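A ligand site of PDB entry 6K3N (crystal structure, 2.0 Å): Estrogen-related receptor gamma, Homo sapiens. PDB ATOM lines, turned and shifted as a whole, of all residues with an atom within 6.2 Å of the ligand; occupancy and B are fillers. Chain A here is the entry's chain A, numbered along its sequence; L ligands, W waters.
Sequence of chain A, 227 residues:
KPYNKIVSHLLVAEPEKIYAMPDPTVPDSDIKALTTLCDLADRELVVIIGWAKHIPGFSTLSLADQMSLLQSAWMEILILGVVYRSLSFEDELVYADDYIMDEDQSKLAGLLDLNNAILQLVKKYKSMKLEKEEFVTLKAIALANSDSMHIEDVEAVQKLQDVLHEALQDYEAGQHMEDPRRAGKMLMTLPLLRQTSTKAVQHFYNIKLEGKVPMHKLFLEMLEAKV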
ATOM      1  N   LEU A  34      20.056 -18.738 -14.491  1.00  0.00           N
ATOM      2  CA  LEU A  34      21.391 -18.945 -14.981  1.00  0.00           C
ATOM      3  C   LEU A  34      21.440 -20.301 -15.719  1.00  0.00           C
ATOM      4  O   LEU A  34      22.146 -20.432 -16.676  1.00  0.00           O
ATOM      5  CB  LEU A  34      22.456 -18.879 -13.853  1.00  0.00           C
ATOM      6  CG  LEU A  34      22.667 -17.484 -13.163  1.00  0.00           C
ATOM      7  CD1 LEU A  34      23.560 -17.726 -11.947  1.00  0.00           C
ATOM      8  CD2 LEU A  34      23.330 -16.476 -14.141  1.00  0.00           C
ATOM      9  N   LEU A  37      19.717 -19.656 -19.142  1.00  0.00           N
ATOM     10  CA  LEU A  37      20.632 -18.923 -20.033  1.00  0.00           C
ATOM     11  C   LEU A  37      21.829 -19.704 -20.543  1.00  0.00           C
ATOM     12  O   LEU A  37      22.160 -19.534 -21.717  1.00  0.00           O
ATOM     13  CB  LEU A  37      21.146 -17.646 -19.344  1.00  0.00           C
ATOM     14  CG  LEU A  37      20.055 -16.616 -19.108  1.00  0.00           C
ATOM     15  CD1 LEU A  37      20.395 -15.584 -18.026  1.00  0.00           C
ATOM     16  CD2 LEU A  37      19.518 -15.964 -20.377  1.00  0.00           C
ATOM     17  N   CYS A  38      22.511 -20.495 -19.711  1.00  0.00           N
ATOM     18  CA  CYS A  38      23.663 -21.267 -20.184  1.00  0.00           C
ATOM     19  C   CYS A  38      23.210 -22.454 -21.006  1.00  0.00           C
ATOM     20  O   CYS A  38      23.939 -22.903 -21.909  1.00  0.00           O
ATOM     21  CB  CYS A  38      24.499 -21.800 -19.030  1.00  0.00           C
ATOM     22  SG  CYS A  38      25.168 -20.460 -18.027  1.00  0.00           S
ATOM     23  N   LEU A  40      20.407 -22.295 -23.155  1.00  0.00           N
ATOM     24  CA  LEU A  40      20.232 -21.584 -24.381  1.00  0.00           C
ATOM     25  C   LEU A  40      21.561 -21.322 -25.085  1.00  0.00           C
ATOM     26  O   LEU A  40      21.696 -21.676 -26.262  1.00  0.00           O
ATOM     27  CB  LEU A  40      19.567 -20.245 -24.121  1.00  0.00           C
ATOM     28  CG  LEU A  40      19.361 -19.375 -25.316  1.00  0.00           C
ATOM     29  CD1 LEU A  40      18.352 -19.991 -26.353  1.00  0.00           C
ATOM     30  CD2 LEU A  40      18.949 -17.991 -24.822  1.00  0.00           C
ATOM     31  N   ALA A  41      22.522 -20.717 -24.390  1.00  0.00           N
ATOM     32  CA  ALA A  41      23.871 -20.519 -24.967  1.00  0.00           C
ATOM     33  C   ALA A  41      24.412 -21.831 -25.581  1.00  0.00           C
ATOM     34  O   ALA A  41      24.948 -21.851 -26.699  1.00  0.00           O
ATOM     35  CB  ALA A  41      24.847 -20.023 -23.896  1.00  0.00           C
ATOM     36  N   GLU A  44      22.673 -22.348 -28.776  1.00  0.00           N
ATOM     37  CA  GLU A  44      23.078 -21.384 -29.770  1.00  0.00           C
ATOM     38  C   GLU A  44      24.485 -21.690 -30.260  1.00  0.00           C
ATOM     39  O   GLU A  44      24.759 -21.516 -31.460  1.00  0.00           O
ATOM     40  CB  GLU A  44      23.007 -19.942 -29.210  1.00  0.00           C
ATOM     41  CG  GLU A  44      21.570 -19.477 -29.020  1.00  0.00           C
ATOM     42  CD  GLU A  44      21.562 -18.057 -28.612  1.00  0.00           C
ATOM     43  OE1 GLU A  44      21.975 -17.276 -29.438  1.00  0.00           O
ATOM     44  OE2 GLU A  44      21.279 -17.771 -27.458  1.00  0.00           O
ATOM     45  N   TRP A  74      33.229 -16.730 -29.373  1.00  0.00           N
ATOM     46  CA  TRP A  74      31.866 -17.180 -29.105  1.00  0.00           C
ATOM     47  C   TRP A  74      31.049 -16.213 -28.282  1.00  0.00           C
ATOM     48  O   TRP A  74      29.916 -15.981 -28.607  1.00  0.00           O
ATOM     49  CB  TRP A  74      31.787 -18.555 -28.519  1.00  0.00           C
ATOM     50  CG  TRP A  74      32.387 -18.621 -27.129  1.00  0.00           C
ATOM     51  CD1 TRP A  74      33.721 -18.570 -26.751  1.00  0.00           C
ATOM     52  CD2 TRP A  74      31.645 -18.633 -25.885  1.00  0.00           C
ATOM     53  NE1 TRP A  74      33.854 -18.570 -25.375  1.00  0.00           N
ATOM     54  CE2 TRP A  74      32.629 -18.641 -24.794  1.00  0.00           C
ATOM     55  CE3 TRP A  74      30.294 -18.684 -25.568  1.00  0.00           C
ATOM     56  CZ2 TRP A  74      32.254 -18.734 -23.462  1.00  0.00           C
ATOM     57  CZ3 TRP A  74      29.945 -18.755 -24.227  1.00  0.00           C
ATOM     58  CH2 TRP A  74      30.898 -18.785 -23.198  1.00  0.00           C
ATOM     59  N   MET A  75      31.597 -15.678 -27.200  1.00  0.00           N
ATOM     60  CA  MET A  75      30.818 -14.823 -26.358  1.00  0.00           C
ATOM     61  C   MET A  75      30.411 -13.531 -27.053  1.00  0.00           C
ATOM     62  O   MET A  75      29.324 -13.058 -26.882  1.00  0.00           O
ATOM     63  CB  MET A  75      31.505 -14.601 -25.016  1.00  0.00           C
ATOM     64  CG  MET A  75      30.795 -13.638 -24.145  1.00  0.00           C
ATOM     65  SD  MET A  75      29.370 -14.475 -23.372  1.00  0.00           S
ATOM     66  CE  MET A  75      30.323 -15.426 -22.156  1.00  0.00           C
ATOM     67  N   LEU A  78      27.422 -14.359 -29.207  1.00  0.00           N
ATOM     68  CA  LEU A  78      26.204 -14.560 -28.428  1.00  0.00           C
ATOM     69  C   LEU A  78      25.623 -13.228 -28.050  1.00  0.00           C
ATOM     70  O   LEU A  78      24.415 -13.014 -28.132  1.00  0.00           O
ATOM     71  CB  LEU A  78      26.505 -15.411 -27.166  1.00  0.00           C
ATOM     72  CG  LEU A  78      26.618 -16.944 -27.404  1.00  0.00           C
ATOM     73  CD1 LEU A  78      26.932 -17.637 -26.098  1.00  0.00           C
ATOM     74  CD2 LEU A  78      25.308 -17.522 -27.981  1.00  0.00           C
ATOM     75  N   ILE A  79      26.491 -12.331 -27.625  1.00  0.00           N
ATOM     76  CA  ILE A  79      26.016 -11.019 -27.037  1.00  0.00           C
ATOM     77  C   ILE A  79      25.455 -10.130 -28.125  1.00  0.00           C
ATOM     78  O   ILE A  79      24.412  -9.574 -27.950  1.00  0.00           O
ATOM     79  CB  ILE A  79      27.128 -10.333 -26.274  1.00  0.00           C
ATOM     80  CG1 ILE A  79      27.320 -11.122 -24.966  1.00  0.00           C
ATOM     81  CG2 ILE A  79      26.795  -8.818 -25.996  1.00  0.00           C
ATOM     82  CD1 ILE A  79      28.421 -10.580 -24.080  1.00  0.00           C
ATOM     83  N   GLY A  81      24.073 -11.174 -30.752  1.00  0.00           N
ATOM     84  CA  GLY A  81      22.681 -11.739 -31.012  1.00  0.00           C
ATOM     85  C   GLY A  81      21.631 -11.154 -30.052  1.00  0.00           C
ATOM     86  O   GLY A  81      20.684 -10.562 -30.529  1.00  0.00           O
ATOM     87  N   VAL A  82      21.799 -11.294 -28.724  1.00  0.00           N
ATOM     88  CA  VAL A  82      20.812 -10.703 -27.756  1.00  0.00           C
ATOM     89  C   VAL A  82      20.657  -9.158 -27.936  1.00  0.00           C
ATOM     90  O   VAL A  82      19.518  -8.651 -27.909  1.00  0.00           O
ATOM     91  CB  VAL A  82      21.013 -11.095 -26.245  1.00  0.00           C
ATOM     92  CG1 VAL A  82      22.392 -10.736 -25.697  1.00  0.00           C
ATOM     93  CG2 VAL A  82      19.872 -10.511 -25.367  1.00  0.00           C
ATOM     94  N   ARG A  85      18.541  -8.658 -31.044  1.00  0.00           N
ATOM     95  CA  ARG A  85      17.140  -8.988 -30.838  1.00  0.00           C
ATOM     96  C   ARG A  85      16.500  -7.971 -29.939  1.00  0.00           C
ATOM     97  O   ARG A  85      15.263  -7.877 -29.887  1.00  0.00           O
ATOM     98  CB  ARG A  85      17.054 -10.327 -30.159  1.00  0.00           C
ATOM     99  CG  ARG A  85      17.510 -11.451 -31.081  1.00  0.00           C
ATOM    100  CD  ARG A  85      17.166 -12.792 -30.362  1.00  0.00           C
ATOM    101  NE  ARG A  85      17.960 -13.089 -29.157  1.00  0.00           N
ATOM    102  CZ  ARG A  85      19.163 -13.652 -29.133  1.00  0.00           C
ATOM    103  NH1 ARG A  85      19.848 -13.864 -30.240  1.00  0.00           N
ATOM    104  NH2 ARG A  85      19.741 -13.974 -28.000  1.00  0.00           N
ATOM    105  N   LEU A  93      16.213  -7.196 -22.355  1.00  0.00           N
ATOM    106  CA  LEU A  93      17.056  -7.977 -23.291  1.00  0.00           C
ATOM    107  C   LEU A  93      16.357  -9.299 -23.744  1.00  0.00           C
ATOM    108  O   LEU A  93      16.041 -10.161 -22.925  1.00  0.00           O
ATOM    109  CB  LEU A  93      18.318  -8.371 -22.579  1.00  0.00           C
ATOM    110  CG  LEU A  93      19.171  -7.097 -22.291  1.00  0.00           C
ATOM    111  CD1 LEU A  93      20.340  -7.519 -21.395  1.00  0.00           C
ATOM    112  CD2 LEU A  93      19.681  -6.558 -23.635  1.00  0.00           C
ATOM    113  N   TYR A  95      16.754 -12.368 -24.753  1.00  0.00           N
ATOM    114  CA  TYR A  95      17.546 -13.577 -24.863  1.00  0.00           C
ATOM    115  C   TYR A  95      16.860 -14.561 -25.826  1.00  0.00           C
ATOM    116  O   TYR A  95      17.545 -15.215 -26.631  1.00  0.00           O
ATOM    117  CB  TYR A  95      17.916 -14.229 -23.502  1.00  0.00           C
ATOM    118  CG  TYR A  95      19.005 -13.412 -22.844  1.00  0.00           C
ATOM    119  CD1 TYR A  95      18.670 -12.325 -21.972  1.00  0.00           C
ATOM    120  CD2 TYR A  95      20.323 -13.561 -23.269  1.00  0.00           C
ATOM    121  CE1 TYR A  95      19.696 -11.548 -21.421  1.00  0.00           C
ATOM    122  CE2 TYR A  95      21.371 -12.785 -22.758  1.00  0.00           C
ATOM    123  CZ  TYR A  95      21.044 -11.757 -21.851  1.00  0.00           C
ATOM    124  OH  TYR A  95      22.085 -10.925 -21.393  1.00  0.00           O
ATOM    125  N   MET A 101      14.567 -10.549 -20.382  1.00  0.00           N
ATOM    126  CA  MET A 101      15.018 -10.176 -19.042  1.00  0.00           C
ATOM    127  C   MET A 101      14.824  -8.673 -18.813  1.00  0.00           C
ATOM    128  O   MET A 101      15.353  -7.869 -19.550  1.00  0.00           O
ATOM    129  CB  MET A 101      16.483 -10.555 -18.818  1.00  0.00           C
ATOM    130  CG  MET A 101      16.707 -12.039 -18.877  1.00  0.00           C
ATOM    131  SD  MET A 101      18.291 -12.479 -18.198  1.00  0.00           S
ATOM    132  CE  MET A 101      17.977 -12.112 -16.460  1.00  0.00           C
ATOM    133  N   LEU A 111      22.935 -10.648 -12.551  1.00  0.00           N
ATOM    134  CA  LEU A 111      23.394 -10.251 -13.893  1.00  0.00           C
ATOM    135  C   LEU A 111      23.099  -8.768 -14.132  1.00  0.00           C
ATOM    136  O   LEU A 111      23.175  -8.270 -15.285  1.00  0.00           O
ATOM    137  CB  LEU A 111      22.680 -11.127 -14.962  1.00  0.00           C
ATOM    138  CG  LEU A 111      23.116 -12.595 -15.008  1.00  0.00           C
ATOM    139  CD1 LEU A 111      22.191 -13.469 -15.906  1.00  0.00           C
ATOM    140  CD2 LEU A 111      24.538 -12.616 -15.513  1.00  0.00           C
ATOM    141  N   LEU A 114      26.223  -6.930 -15.827  1.00  0.00           N
ATOM    142  CA  LEU A 114      26.516  -7.350 -17.225  1.00  0.00           C
ATOM    143  C   LEU A 114      25.376  -6.981 -18.138  1.00  0.00           C
ATOM    144  O   LEU A 114      25.622  -6.477 -19.247  1.00  0.00           O
ATOM    145  CB  LEU A 114      26.738  -8.853 -17.392  1.00  0.00           C
ATOM    146  CG  LEU A 114      28.075  -9.524 -17.228  1.00  0.00           C
ATOM    147  CD1 LEU A 114      27.829 -11.024 -17.291  1.00  0.00           C
ATOM    148  CD2 LEU A 114      29.060  -9.051 -18.281  1.00  0.00           C
ATOM    149  N   ASN A 115      24.133  -7.251 -17.711  1.00  0.00           N
ATOM    150  CA  ASN A 115      23.016  -6.899 -18.578  1.00  0.00           C
ATOM    151  C   ASN A 115      22.936  -5.424 -18.799  1.00  0.00           C
ATOM    152  O   ASN A 115      22.516  -4.972 -19.874  1.00  0.00           O
ATOM    153  CB  ASN A 115      21.683  -7.445 -18.084  1.00  0.00           C
ATOM    154  CG  ASN A 115      21.506  -8.926 -18.442  1.00  0.00           C
ATOM    155  OD1 ASN A 115      22.290  -9.475 -19.251  1.00  0.00           O
ATOM    156  ND2 ASN A 115      20.521  -9.582 -17.800  1.00  0.00           N
ATOM    157  N   ILE A 118      25.294  -4.748 -21.508  1.00  0.00           N
ATOM    158  CA  ILE A 118      24.738  -5.193 -22.797  1.00  0.00           C
ATOM    159  C   ILE A 118      23.700  -4.174 -23.223  1.00  0.00           C
ATOM    160  O   ILE A 118      23.577  -3.833 -24.366  1.00  0.00           O
ATOM    161  CB  ILE A 118      24.110  -6.605 -22.645  1.00  0.00           C
ATOM    162  CG1 ILE A 118      25.234  -7.604 -22.336  1.00  0.00           C
ATOM    163  CG2 ILE A 118      23.281  -6.945 -23.893  1.00  0.00           C
ATOM    164  CD1 ILE A 118      24.805  -9.098 -22.228  1.00  0.00           C
ATOM    165  N   ALA A 200      31.789 -10.948 -19.352  1.00  0.00           N
ATOM    166  CA  ALA A 200      30.790 -11.999 -19.298  1.00  0.00           C
ATOM    167  C   ALA A 200      31.487 -13.338 -19.144  1.00  0.00           C
ATOM    168  O   ALA A 200      31.067 -14.169 -18.308  1.00  0.00           O
ATOM    169  CB  ALA A 200      29.872 -11.985 -20.505  1.00  0.00           C
ATOM    170  N   PHE A 204      30.942 -15.900 -15.976  1.00  0.00           N
ATOM    171  CA  PHE A 204      30.419 -17.242 -16.145  1.00  0.00           C
ATOM    172  C   PHE A 204      31.459 -18.307 -15.793  1.00  0.00           C
ATOM    173  O   PHE A 204      31.112 -19.391 -15.332  1.00  0.00           O
ATOM    174  CB  PHE A 204      29.762 -17.419 -17.553  1.00  0.00           C
ATOM    175  CG  PHE A 204      28.326 -16.871 -17.598  1.00  0.00           C
ATOM    176  CD1 PHE A 204      28.054 -15.570 -18.017  1.00  0.00           C
ATOM    177  CD2 PHE A 204      27.253 -17.625 -17.142  1.00  0.00           C
ATOM    178  CE1 PHE A 204      26.759 -15.057 -18.059  1.00  0.00           C
ATOM    179  CE2 PHE A 204      25.964 -17.110 -17.160  1.00  0.00           C
ATOM    180  CZ  PHE A 204      25.700 -15.812 -17.619  1.00  0.00           C
ATOM    181  N   PHE A 219      29.163 -25.457 -24.121  1.00  0.00           N
ATOM    182  CA  PHE A 219      29.320 -24.198 -23.365  1.00  0.00           C
ATOM    183  C   PHE A 219      30.516 -24.311 -22.412  1.00  0.00           C
ATOM    184  O   PHE A 219      31.316 -23.385 -22.328  1.00  0.00           O
ATOM    185  CB  PHE A 219      28.034 -23.927 -22.579  1.00  0.00           C
ATOM    186  CG  PHE A 219      28.004 -22.607 -21.827  1.00  0.00           C
ATOM    187  CD1 PHE A 219      27.719 -21.428 -22.476  1.00  0.00           C
ATOM    188  CD2 PHE A 219      28.222 -22.555 -20.440  1.00  0.00           C
ATOM    189  CE1 PHE A 219      27.661 -20.199 -21.778  1.00  0.00           C
ATOM    190  CE2 PHE A 219      28.164 -21.332 -19.729  1.00  0.00           C
ATOM    191  CZ  PHE A 219      27.866 -20.158 -20.395  1.00  0.00           C
HETATM  192  F1  LIG L   1      22.605 -12.595 -19.223  1.00  0.00           F
HETATM  193  C1  LIG L   1      23.716 -12.911 -19.844  1.00  0.00           C
HETATM  194  C2  LIG L   1      23.774 -14.144 -20.482  1.00  0.00           C
HETATM  195  C3  LIG L   1      24.944 -14.471 -21.157  1.00  0.00           C
HETATM  196  C4  LIG L   1      25.995 -13.539 -21.149  1.00  0.00           C
HETATM  197  C5  LIG L   1      25.955 -12.284 -20.479  1.00  0.00           C
HETATM  198  C6  LIG L   1      24.781 -11.979 -19.806  1.00  0.00           C
HETATM  199  O1  LIG L   1      24.609 -10.809 -19.090  1.00  0.00           O
HETATM  200  C7  LIG L   1      25.014 -15.821 -21.900  1.00  0.00           C
HETATM  201  C8  LIG L   1      26.448 -16.130 -22.346  1.00  0.00           C
HETATM  202  C9  LIG L   1      24.714 -17.004 -20.975  1.00  0.00           C
HETATM  203  C10 LIG L   1      24.141 -15.762 -23.143  1.00  0.00           C
HETATM  204  C11 LIG L   1      24.313 -14.688 -24.018  1.00  0.00           C
HETATM  205  C12 LIG L   1      23.564 -14.615 -25.199  1.00  0.00           C
HETATM  206  C13 LIG L   1      22.658 -15.606 -25.547  1.00  0.00           C
HETATM  207  O2  LIG L   1      21.992 -15.450 -26.764  1.00  0.00           O
HETATM  208  C14 LIG L   1      22.486 -16.726 -24.669  1.00  0.00           C
HETATM  209  C15 LIG L   1      23.181 -16.776 -23.484  1.00  0.00           C
HETATM  210  O   HOH W   1      22.672 -14.717 -29.566  1.00  0.00           O
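OH of Tyr 95 lies close to O1 of the ligand (3.4 Å).
An oxygen (O1) of the ligand lies within hydrogen-bond range of the side-chain amide oxygen of Asn 115 (2.7 Å).
An oxygen (O2) of the ligand is in hydrogen-bond range of the side-chain carboxylate (OE2) of Glu 44 (2.5 Å).
The guanidinium group of Arg 85 is in hydrogen-bond range of an oxygen (O2) of the ligand.
O of Tyr 95 lies within hydrogen-bond range of NH2 of Arg 85 (2.9 Å).
The side-chain sulfur (SD) of Met 101 sits at hydrogen-bond distance from the side-chain amide nitrogen (ND2) of Asn 115.
NH1 of Arg 85 sits close to O of Gly 81 (3.4 Å).
OD1 of Asn 115 is in hydrogen-bond range of OH of Tyr 95.
O of Leu 37 touches C15 of the ligand (3.4 Å).
Leu 40 touches the ligand (CD2 to C14, 3.8 Å).
Ala 41 touches the ligand (CB to C15, 3.7 Å).
Met 75 touches the ligand.
Leu 78 touches the ligand.
Leu 111 touches the ligand (CD1 to F1, 3.5 Å).
Leu 114 touches the ligand (CB to O1, 3.4 Å).
Ile 118 touches the ligand (CD1 to O1, 3.6 Å).
CB of Ala 200 touches C5 of the ligand (3.9 Å).
CE1 of Phe 204 touches C4 of the ligand, at 3.5 Å.
Within 4 Å of the ligand: Leu 37, Leu 40, Ala 41, Glu 44, Met 75, Leu 78, Arg 85, Tyr 95, Leu 111, Leu 114, Asn 115, Ile 118, Ala 200 and Phe 204.
The nearest printed residue that does not touch the ligand is Val 82 (4.1 Å).
Water W1 lies within hydrogen-bond range of the side-chain carboxylate of Glu 44 (2.7 Å), the backbone carbonyl oxygen of Leu 78 (2.8 Å), an oxygen (O2) of the ligand (3.0 Å) and the guanidinium group of Arg 85 (3.0 Å).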
